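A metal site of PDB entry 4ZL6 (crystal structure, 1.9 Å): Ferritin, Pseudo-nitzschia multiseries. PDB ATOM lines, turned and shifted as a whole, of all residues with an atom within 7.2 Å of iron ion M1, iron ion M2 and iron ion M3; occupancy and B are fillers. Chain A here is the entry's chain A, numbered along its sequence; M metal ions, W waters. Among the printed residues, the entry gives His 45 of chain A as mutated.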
ATOM      1  N   GLN A  12       7.930  14.610  16.277  1.00  0.00           N
ATOM      2  CA  GLN A  12       7.957  15.267  14.976  1.00  0.00           C
ATOM      3  C   GLN A  12       8.785  14.487  13.950  1.00  0.00           C
ATOM      4  O   GLN A  12       8.401  14.354  12.813  1.00  0.00           O
ATOM      5  CB  GLN A  12       8.458  16.687  15.103  1.00  0.00           C
ATOM      6  CG  GLN A  12       8.257  17.441  13.803  1.00  0.00           C
ATOM      7  CD  GLN A  12       6.782  17.562  13.494  1.00  0.00           C
ATOM      8  OE1 GLN A  12       5.967  17.647  14.412  1.00  0.00           O
ATOM      9  NE2 GLN A  12       6.426  17.503  12.250  1.00  0.00           N
ATOM     10  N   GLN A  15       6.662  11.683  12.913  1.00  0.00           N
ATOM     11  CA  GLN A  15       5.588  12.220  12.033  1.00  0.00           C
ATOM     12  C   GLN A  15       6.118  12.385  10.610  1.00  0.00           C
ATOM     13  O   GLN A  15       5.424  12.012   9.619  1.00  0.00           O
ATOM     14  CB  GLN A  15       5.074  13.511  12.579  1.00  0.00           C
ATOM     15  CG  GLN A  15       3.972  14.145  11.766  1.00  0.00           C
ATOM     16  CD  GLN A  15       2.760  13.213  11.624  1.00  0.00           C
ATOM     17  OE1 GLN A  15       2.314  12.589  12.640  1.00  0.00           O
ATOM     18  NE2 GLN A  15       2.278  13.027  10.356  1.00  0.00           N
ATOM     19  N   GLU A  16       7.352  12.908  10.480  1.00  0.00           N
ATOM     20  CA  GLU A  16       7.930  13.095   9.150  1.00  0.00           C
ATOM     21  C   GLU A  16       8.185  11.755   8.468  1.00  0.00           C
ATOM     22  O   GLU A  16       7.819  11.590   7.264  1.00  0.00           O
ATOM     23  CB  GLU A  16       9.220  13.878   9.198  1.00  0.00           C
ATOM     24  CG  GLU A  16       9.114  15.291   9.766  1.00  0.00           C
ATOM     25  CD  GLU A  16       8.246  16.214   8.908  1.00  0.00           C
ATOM     26  OE1 GLU A  16       8.030  15.942   7.716  1.00  0.00           O
ATOM     27  OE2 GLU A  16       7.747  17.180   9.468  1.00  0.00           O
ATOM     28  N   ALA A  19       4.779  10.212   7.433  1.00  0.00           N
ATOM     29  CA  ALA A  19       4.315  10.869   6.216  1.00  0.00           C
ATOM     30  C   ALA A  19       5.077  10.409   4.980  1.00  0.00           C
ATOM     31  O   ALA A  19       4.460  10.176   3.892  1.00  0.00           O
ATOM     32  CB  ALA A  19       4.368  12.422   6.392  1.00  0.00           C
ATOM     33  N   SER A  20       6.385  10.191   5.117  1.00  0.00           N
ATOM     34  CA  SER A  20       7.183   9.635   4.019  1.00  0.00           C
ATOM     35  C   SER A  20       6.625   8.310   3.540  1.00  0.00           C
ATOM     36  O   SER A  20       6.513   8.062   2.359  1.00  0.00           O
ATOM     37  CB  SER A  20       8.641   9.467   4.411  1.00  0.00           C
ATOM     38  OG  SER A  20       9.360   9.013   3.338  1.00  0.00           O
ATOM     39  N   TYR A  23       3.155   8.927   1.677  1.00  0.00           N
ATOM     40  CA  TYR A  23       3.541   9.284   0.262  1.00  0.00           C
ATOM     41  C   TYR A  23       4.017   8.137  -0.603  1.00  0.00           C
ATOM     42  O   TYR A  23       3.582   7.979  -1.730  1.00  0.00           O
ATOM     43  CB  TYR A  23       4.556  10.392   0.278  1.00  0.00           C
ATOM     44  CG  TYR A  23       3.957  11.750   0.488  1.00  0.00           C
ATOM     45  CD1 TYR A  23       3.282  12.399  -0.546  1.00  0.00           C
ATOM     46  CD2 TYR A  23       4.154  12.456   1.666  1.00  0.00           C
ATOM     47  CE1 TYR A  23       2.744  13.676  -0.392  1.00  0.00           C
ATOM     48  CE2 TYR A  23       3.605  13.705   1.843  1.00  0.00           C
ATOM     49  CZ  TYR A  23       2.906  14.320   0.809  1.00  0.00           C
ATOM     50  OH  TYR A  23       2.380  15.567   0.990  1.00  0.00           O
ATOM     51  N   TYR A  41       5.186  12.318  -8.564  1.00  0.00           N
ATOM     52  CA  TYR A  41       5.024  13.409  -7.642  1.00  0.00           C
ATOM     53  C   TYR A  41       5.099  12.853  -6.187  1.00  0.00           C
ATOM     54  O   TYR A  41       5.737  13.416  -5.303  1.00  0.00           O
ATOM     55  CB  TYR A  41       3.689  14.132  -7.812  1.00  0.00           C
ATOM     56  CG  TYR A  41       3.457  15.182  -6.722  1.00  0.00           C
ATOM     57  CD1 TYR A  41       2.911  14.825  -5.522  1.00  0.00           C
ATOM     58  CD2 TYR A  41       3.834  16.523  -6.870  1.00  0.00           C
ATOM     59  CE1 TYR A  41       2.757  15.712  -4.487  1.00  0.00           C
ATOM     60  CE2 TYR A  41       3.651  17.444  -5.823  1.00  0.00           C
ATOM     61  CZ  TYR A  41       3.133  17.016  -4.631  1.00  0.00           C
ATOM     62  OH  TYR A  41       2.962  17.821  -3.486  1.00  0.00           O
ATOM     63  N   HIS A  45       7.840  13.525  -3.175  1.00  0.00           N
ATOM     64  CA  HIS A  45       7.439  14.038  -1.918  1.00  0.00           C
ATOM     65  C   HIS A  45       7.770  13.095  -0.770  1.00  0.00           C
ATOM     66  O   HIS A  45       8.194  13.546   0.327  1.00  0.00           O
ATOM     67  CB  HIS A  45       5.967  14.428  -1.939  1.00  0.00           C
ATOM     68  CG  HIS A  45       5.636  15.507  -0.972  1.00  0.00           C
ATOM     69  ND1 HIS A  45       4.882  16.612  -1.315  1.00  0.00           N
ATOM     70  CD2 HIS A  45       6.026  15.696   0.320  1.00  0.00           C
ATOM     71  CE1 HIS A  45       4.746  17.379  -0.243  1.00  0.00           C
ATOM     72  NE2 HIS A  45       5.452  16.858   0.756  1.00  0.00           N
ATOM     73  N   GLU A  48      11.238  13.915   0.166  1.00  0.00           N
ATOM     74  CA  GLU A  48      11.273  15.191   0.803  1.00  0.00           C
ATOM     75  C   GLU A  48      10.830  15.080   2.277  1.00  0.00           C
ATOM     76  O   GLU A  48      11.470  15.735   3.140  1.00  0.00           O
ATOM     77  CB  GLU A  48      10.388  16.167   0.045  1.00  0.00           C
ATOM     78  CG  GLU A  48      10.243  17.461   0.757  1.00  0.00           C
ATOM     79  CD  GLU A  48       9.540  18.527  -0.078  1.00  0.00           C
ATOM     80  OE1 GLU A  48       9.638  18.491  -1.350  1.00  0.00           O
ATOM     81  OE2 GLU A  48       8.884  19.378   0.563  1.00  0.00           O
ATOM     82  N   GLU A  49       9.779  14.303   2.567  1.00  0.00           N
ATOM     83  CA  GLU A  49       9.384  14.125   3.996  1.00  0.00           C
ATOM     84  C   GLU A  49      10.521  13.498   4.804  1.00  0.00           C
ATOM     85  O   GLU A  49      10.764  13.855   5.987  1.00  0.00           O
ATOM     86  CB  GLU A  49       8.170  13.224   4.146  1.00  0.00           C
ATOM     87  CG  GLU A  49       6.956  13.700   3.554  1.00  0.00           C
ATOM     88  CD  GLU A  49       6.503  15.051   4.140  1.00  0.00           C
ATOM     89  OE1 GLU A  49       6.774  15.445   5.220  1.00  0.00           O
ATOM     90  OE2 GLU A  49       5.773  15.681   3.477  1.00  0.00           O
ATOM     91  N   ARG A  50      11.178  12.514   4.197  1.00  0.00           N
ATOM     92  CA  ARG A  50      12.291  11.900   4.913  1.00  0.00           C
ATOM     93  C   ARG A  50      13.401  12.926   5.164  1.00  0.00           C
ATOM     94  O   ARG A  50      13.961  12.997   6.285  1.00  0.00           O
ATOM     95  CB  ARG A  50      12.821  10.720   4.122  1.00  0.00           C
ATOM     96  CG  ARG A  50      13.956  10.033   4.842  1.00  0.00           C
ATOM     97  CD  ARG A  50      14.236   8.649   4.362  1.00  0.00           C
ATOM     98  NE  ARG A  50      15.491   8.125   4.929  1.00  0.00           N
ATOM     99  CZ  ARG A  50      16.710   8.443   4.455  1.00  0.00           C
ATOM    100  NH1 ARG A  50      16.888   9.287   3.456  1.00  0.00           N
ATOM    101  NH2 ARG A  50      17.752   7.961   5.050  1.00  0.00           N
ATOM    102  N   HIS A  52      13.036  16.133   5.590  1.00  0.00           N
ATOM    103  CA  HIS A  52      12.607  16.900   6.755  1.00  0.00           C
ATOM    104  C   HIS A  52      12.874  16.212   8.073  1.00  0.00           C
ATOM    105  O   HIS A  52      13.355  16.874   9.069  1.00  0.00           O
ATOM    106  CB  HIS A  52      11.140  17.264   6.765  1.00  0.00           C
ATOM    107  CG  HIS A  52      10.693  18.014   5.591  1.00  0.00           C
ATOM    108  ND1 HIS A  52      11.561  18.835   4.885  1.00  0.00           N
ATOM    109  CD2 HIS A  52       9.461  18.194   5.047  1.00  0.00           C
ATOM    110  CE1 HIS A  52      10.891  19.416   3.896  1.00  0.00           C
ATOM    111  NE2 HIS A  52       9.626  19.045   3.985  1.00  0.00           N
ATOM    112  N   GLY A  53      12.579  14.927   8.150  1.00  0.00           N
ATOM    113  CA  GLY A  53      12.837  14.214   9.389  1.00  0.00           C
ATOM    114  C   GLY A  53      14.308  14.200   9.707  1.00  0.00           C
ATOM    115  O   GLY A  53      14.710  14.389  10.892  1.00  0.00           O
ATOM    116  N   PHE A  56      15.340  17.524  11.319  1.00  0.00           N
ATOM    117  CA  PHE A  56      15.021  17.500  12.740  1.00  0.00           C
ATOM    118  C   PHE A  56      16.041  16.688  13.538  1.00  0.00           C
ATOM    119  O   PHE A  56      16.484  17.108  14.625  1.00  0.00           O
ATOM    120  CB  PHE A  56      13.618  17.009  12.985  1.00  0.00           C
ATOM    121  CG  PHE A  56      12.572  18.077  12.796  1.00  0.00           C
ATOM    122  CD1 PHE A  56      12.220  18.507  11.550  1.00  0.00           C
ATOM    123  CD2 PHE A  56      11.957  18.653  13.873  1.00  0.00           C
ATOM    124  CE1 PHE A  56      11.276  19.489  11.350  1.00  0.00           C
ATOM    125  CE2 PHE A  56      11.002  19.663  13.678  1.00  0.00           C
ATOM    126  CZ  PHE A  56      10.663  20.079  12.421  1.00  0.00           C
ATOM    127  N   LEU A  94      -3.017  14.530   5.580  1.00  0.00           N
ATOM    128  CA  LEU A  94      -1.698  14.264   6.104  1.00  0.00           C
ATOM    129  C   LEU A  94      -0.881  15.565   6.325  1.00  0.00           C
ATOM    130  O   LEU A  94      -0.304  15.805   7.448  1.00  0.00           O
ATOM    131  CB  LEU A  94      -0.975  13.366   5.124  1.00  0.00           C
ATOM    132  CG  LEU A  94       0.480  12.974   5.482  1.00  0.00           C
ATOM    133  CD1 LEU A  94       0.496  12.085   6.734  1.00  0.00           C
ATOM    134  CD2 LEU A  94       1.121  12.286   4.319  1.00  0.00           C
ATOM    135  N   GLU A  95      -0.841  16.425   5.285  1.00  0.00           N
ATOM    136  CA  GLU A  95      -0.165  17.710   5.428  1.00  0.00           C
ATOM    137  C   GLU A  95      -0.802  18.589   6.493  1.00  0.00           C
ATOM    138  O   GLU A  95      -0.100  19.176   7.293  1.00  0.00           O
ATOM    139  CB  GLU A  95      -0.013  18.413   4.086  1.00  0.00           C
ATOM    140  CG  GLU A  95       0.964  17.656   3.232  1.00  0.00           C
ATOM    141  CD  GLU A  95       2.418  17.757   3.706  1.00  0.00           C
ATOM    142  OE1 GLU A  95       2.726  18.416   4.730  1.00  0.00           O
ATOM    143  OE2 GLU A  95       3.301  17.154   3.011  1.00  0.00           O
ATOM    144  N   ASN A  98       0.528  17.399   9.632  1.00  0.00           N
ATOM    145  CA  ASN A  98       1.967  17.733   9.712  1.00  0.00           C
ATOM    146  C   ASN A  98       2.006  19.203  10.275  1.00  0.00           C
ATOM    147  O   ASN A  98       2.742  19.524  11.218  1.00  0.00           O
ATOM    148  CB  ASN A  98       2.704  17.665   8.328  1.00  0.00           C
ATOM    149  CG  ASN A  98       3.193  16.216   7.856  1.00  0.00           C
ATOM    150  OD1 ASN A  98       3.133  15.202   8.579  1.00  0.00           O
ATOM    151  ND2 ASN A  98       3.690  16.149   6.552  1.00  0.00           N
ATOM    152  N   LEU A 102       3.496  20.726  13.875  1.00  0.00           N
ATOM    153  CA  LEU A 102       4.543  21.753  13.900  1.00  0.00           C
ATOM    154  C   LEU A 102       4.135  22.885  14.775  1.00  0.00           C
ATOM    155  O   LEU A 102       4.975  23.444  15.517  1.00  0.00           O
ATOM    156  CB  LEU A 102       4.948  22.296  12.506  1.00  0.00           C
ATOM    157  CG  LEU A 102       5.717  21.260  11.697  1.00  0.00           C
ATOM    158  CD1 LEU A 102       5.715  21.628  10.196  1.00  0.00           C
ATOM    159  CD2 LEU A 102       7.153  21.139  12.210  1.00  0.00           C
ATOM    160  N   PHE A 124       9.950  25.759   8.178  1.00  0.00           N
ATOM    161  CA  PHE A 124       9.027  24.657   8.051  1.00  0.00           C
ATOM    162  C   PHE A 124       7.612  25.201   8.142  1.00  0.00           C
ATOM    163  O   PHE A 124       6.762  24.763   7.407  1.00  0.00           O
ATOM    164  CB  PHE A 124       9.259  23.634   9.171  1.00  0.00           C
ATOM    165  CG  PHE A 124      10.561  22.910   9.050  1.00  0.00           C
ATOM    166  CD1 PHE A 124      10.669  21.826   8.156  1.00  0.00           C
ATOM    167  CD2 PHE A 124      11.671  23.323   9.744  1.00  0.00           C
ATOM    168  CE1 PHE A 124      11.902  21.159   8.012  1.00  0.00           C
ATOM    169  CE2 PHE A 124      12.897  22.690   9.584  1.00  0.00           C
ATOM    170  CZ  PHE A 124      13.018  21.613   8.713  1.00  0.00           C
ATOM    171  N   GLN A 127       7.120  26.606   4.636  1.00  0.00           N
ATOM    172  CA  GLN A 127       6.959  25.468   3.721  1.00  0.00           C
ATOM    173  C   GLN A 127       5.573  24.749   3.822  1.00  0.00           C
ATOM    174  O   GLN A 127       4.992  24.373   2.778  1.00  0.00           O
ATOM    175  CB  GLN A 127       8.088  24.460   3.920  1.00  0.00           C
ATOM    176  CG  GLN A 127       7.978  23.267   2.954  1.00  0.00           C
ATOM    177  CD  GLN A 127       9.221  22.374   2.920  1.00  0.00           C
ATOM    178  OE1 GLN A 127       9.475  21.717   1.924  1.00  0.00           O
ATOM    179  NE2 GLN A 127       9.966  22.324   4.038  1.00  0.00           N
ATOM    180  N   GLN A 128       5.054  24.497   5.024  1.00  0.00           N
ATOM    181  CA  GLN A 128       3.726  23.905   5.153  1.00  0.00           C
ATOM    182  C   GLN A 128       2.653  24.731   4.513  1.00  0.00           C
ATOM    183  O   GLN A 128       1.707  24.202   3.927  1.00  0.00           O
ATOM    184  CB  GLN A 128       3.319  23.662   6.609  1.00  0.00           C
ATOM    185  CG  GLN A 128       4.115  22.617   7.294  1.00  0.00           C
ATOM    186  CD  GLN A 128       3.949  21.281   6.589  1.00  0.00           C
ATOM    187  OE1 GLN A 128       4.914  20.750   5.970  1.00  0.00           O
ATOM    188  NE2 GLN A 128       2.677  20.781   6.557  1.00  0.00           N
ATOM    189  N   GLU A 131       2.972  23.933   0.806  1.00  0.00           N
ATOM    190  CA  GLU A 131       2.535  22.572   0.533  1.00  0.00           C
ATOM    191  C   GLU A 131       1.046  22.420   0.639  1.00  0.00           C
ATOM    192  O   GLU A 131       0.436  21.785  -0.254  1.00  0.00           O
ATOM    193  CB  GLU A 131       3.266  21.582   1.504  1.00  0.00           C
ATOM    194  CG  GLU A 131       4.700  21.553   1.076  1.00  0.00           C
ATOM    195  CD  GLU A 131       5.470  20.436   1.708  1.00  0.00           C
ATOM    196  OE1 GLU A 131       4.815  19.505   2.225  1.00  0.00           O
ATOM    197  OE2 GLU A 131       6.702  20.548   1.654  1.00  0.00           O
ATOM    198  N   ILE A 135      -1.080  21.205  -2.673  1.00  0.00           N
ATOM    199  CA  ILE A 135      -1.866  19.975  -2.531  1.00  0.00           C
ATOM    200  C   ILE A 135      -3.318  20.294  -2.766  1.00  0.00           C
ATOM    201  O   ILE A 135      -3.945  19.717  -3.694  1.00  0.00           O
ATOM    202  CB  ILE A 135      -1.722  19.274  -1.167  1.00  0.00           C
ATOM    203  CG1 ILE A 135      -0.352  18.678  -0.940  1.00  0.00           C
ATOM    204  CG2 ILE A 135      -2.769  18.165  -1.015  1.00  0.00           C
ATOM    205  CD1 ILE A 135       0.266  17.989  -2.132  1.00  0.00           C
HETATM  206 FE    FE M   1       5.408  17.625   2.875  1.00  0.00          FE
HETATM  207 FE    FE M   2       6.937  17.206   6.283  1.00  0.00          FE
HETATM  208 FE    FE M   3       8.175  19.877   2.830  1.00  0.00          FE
HETATM  209  O   HOH W   1       5.468  18.424   4.893  1.00  0.00           O
HETATM  210  O   HOH W   2       7.264  18.935   7.543  1.00  0.00           O
HETATM  211  O   HOH W   3       7.577  21.020   5.780  1.00  0.00           O
HETATM  212  O   HOH W   4       7.354  17.884   2.519  1.00  0.00           O
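Water W4 binds iron ion M1, at 2.0 Å.
Iron ion M1 is bound by OE2 of Glu 49 (2.1 Å).
Iron ion M1 is bound by OE1 of Glu 131 (2.1 Å).
OE2 of Glu 95 binds iron ion M1 (2.2 Å).
Iron ion M1 is bound by water W1 (2.2 Å).
Iron ion M1 is bound by a ring nitrogen (NE2) of His 45 (2.3 Å).
Water W1 lies within hydrogen-bond range of OE1 of Gln 128 (2.6 Å), OE1 of Glu 95 (2.7 Å) and ND2 of Asn 98 (3.3 Å).
Water W2 bridges the side-chain carboxylate (OE2) of Glu 16 (2.6 Å) and the side-chain amide oxygen (OE1) of Gln 128 (3.4 Å).
Water W3 lies within hydrogen-bond range of the side-chain amide oxygen of Gln 128 (2.7 Å) and the side-chain amide nitrogen of Gln 127 (3.2 Å).
Iron ion M3 is bound by OE2 of Glu 131, NE2 of His 52, water W4, OE2 of Glu 48 and OE1 of Gln 127.
Iron ion M2 is bound by OE1 of Glu 49 (2.1 Å).
Water W2 binds iron ion M2, 2.2 Å away.
OE1 of Glu 16 is bound to iron ion M2.
Water W1 is bound to iron ion M2 (2.4 Å).
Of the 23 residues printed, 4 come within 4 Å of iron ion M3.
The nearest printed residue that does not touch iron ion M3 is His 45 (4.6 Å).
OE2 of Glu 16 is in hydrogen-bond range of NE2 of Gln 12.
A ring nitrogen (NE2) of His 45 lies close to the side-chain hydroxyl of Tyr 23 (3.3 Å).
ND2 of Asn 98 lies within hydrogen-bond range of OE1 of Glu 95 (3.1 Å).
The side-chain carboxylate of Glu 95 sits at hydrogen-bond distance from the side-chain amide nitrogen of Gln 128, 3.0 Å away.
The side-chain amide oxygen of Asn 98 sits at hydrogen-bond distance from the side-chain amide nitrogen of Gln 15, 2.9 Å away.
OE1 of Glu 49 lies close to ND2 of Asn 98, at 3.4 Å.
A ring nitrogen (ND1) of His 45 is in hydrogen-bond range of the side-chain hydroxyl (OH) of Tyr 41, at 3.1 Å.
The side-chain carboxylate of Glu 95 lies close to the side-chain hydroxyl of Tyr 23, 2.7 Å away.
ND2 of Asn 98 touches iron ion M2, at 3.4 Å.
Of the 23 residues printed, 4 come within 4 Å of iron ion M2.
The nearest printed residue that does not touch iron ion M2 is Gln 128 (4.1 Å).
The nearest printed residue that does not touch iron ion M1 is Tyr 23 (4.1 Å).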
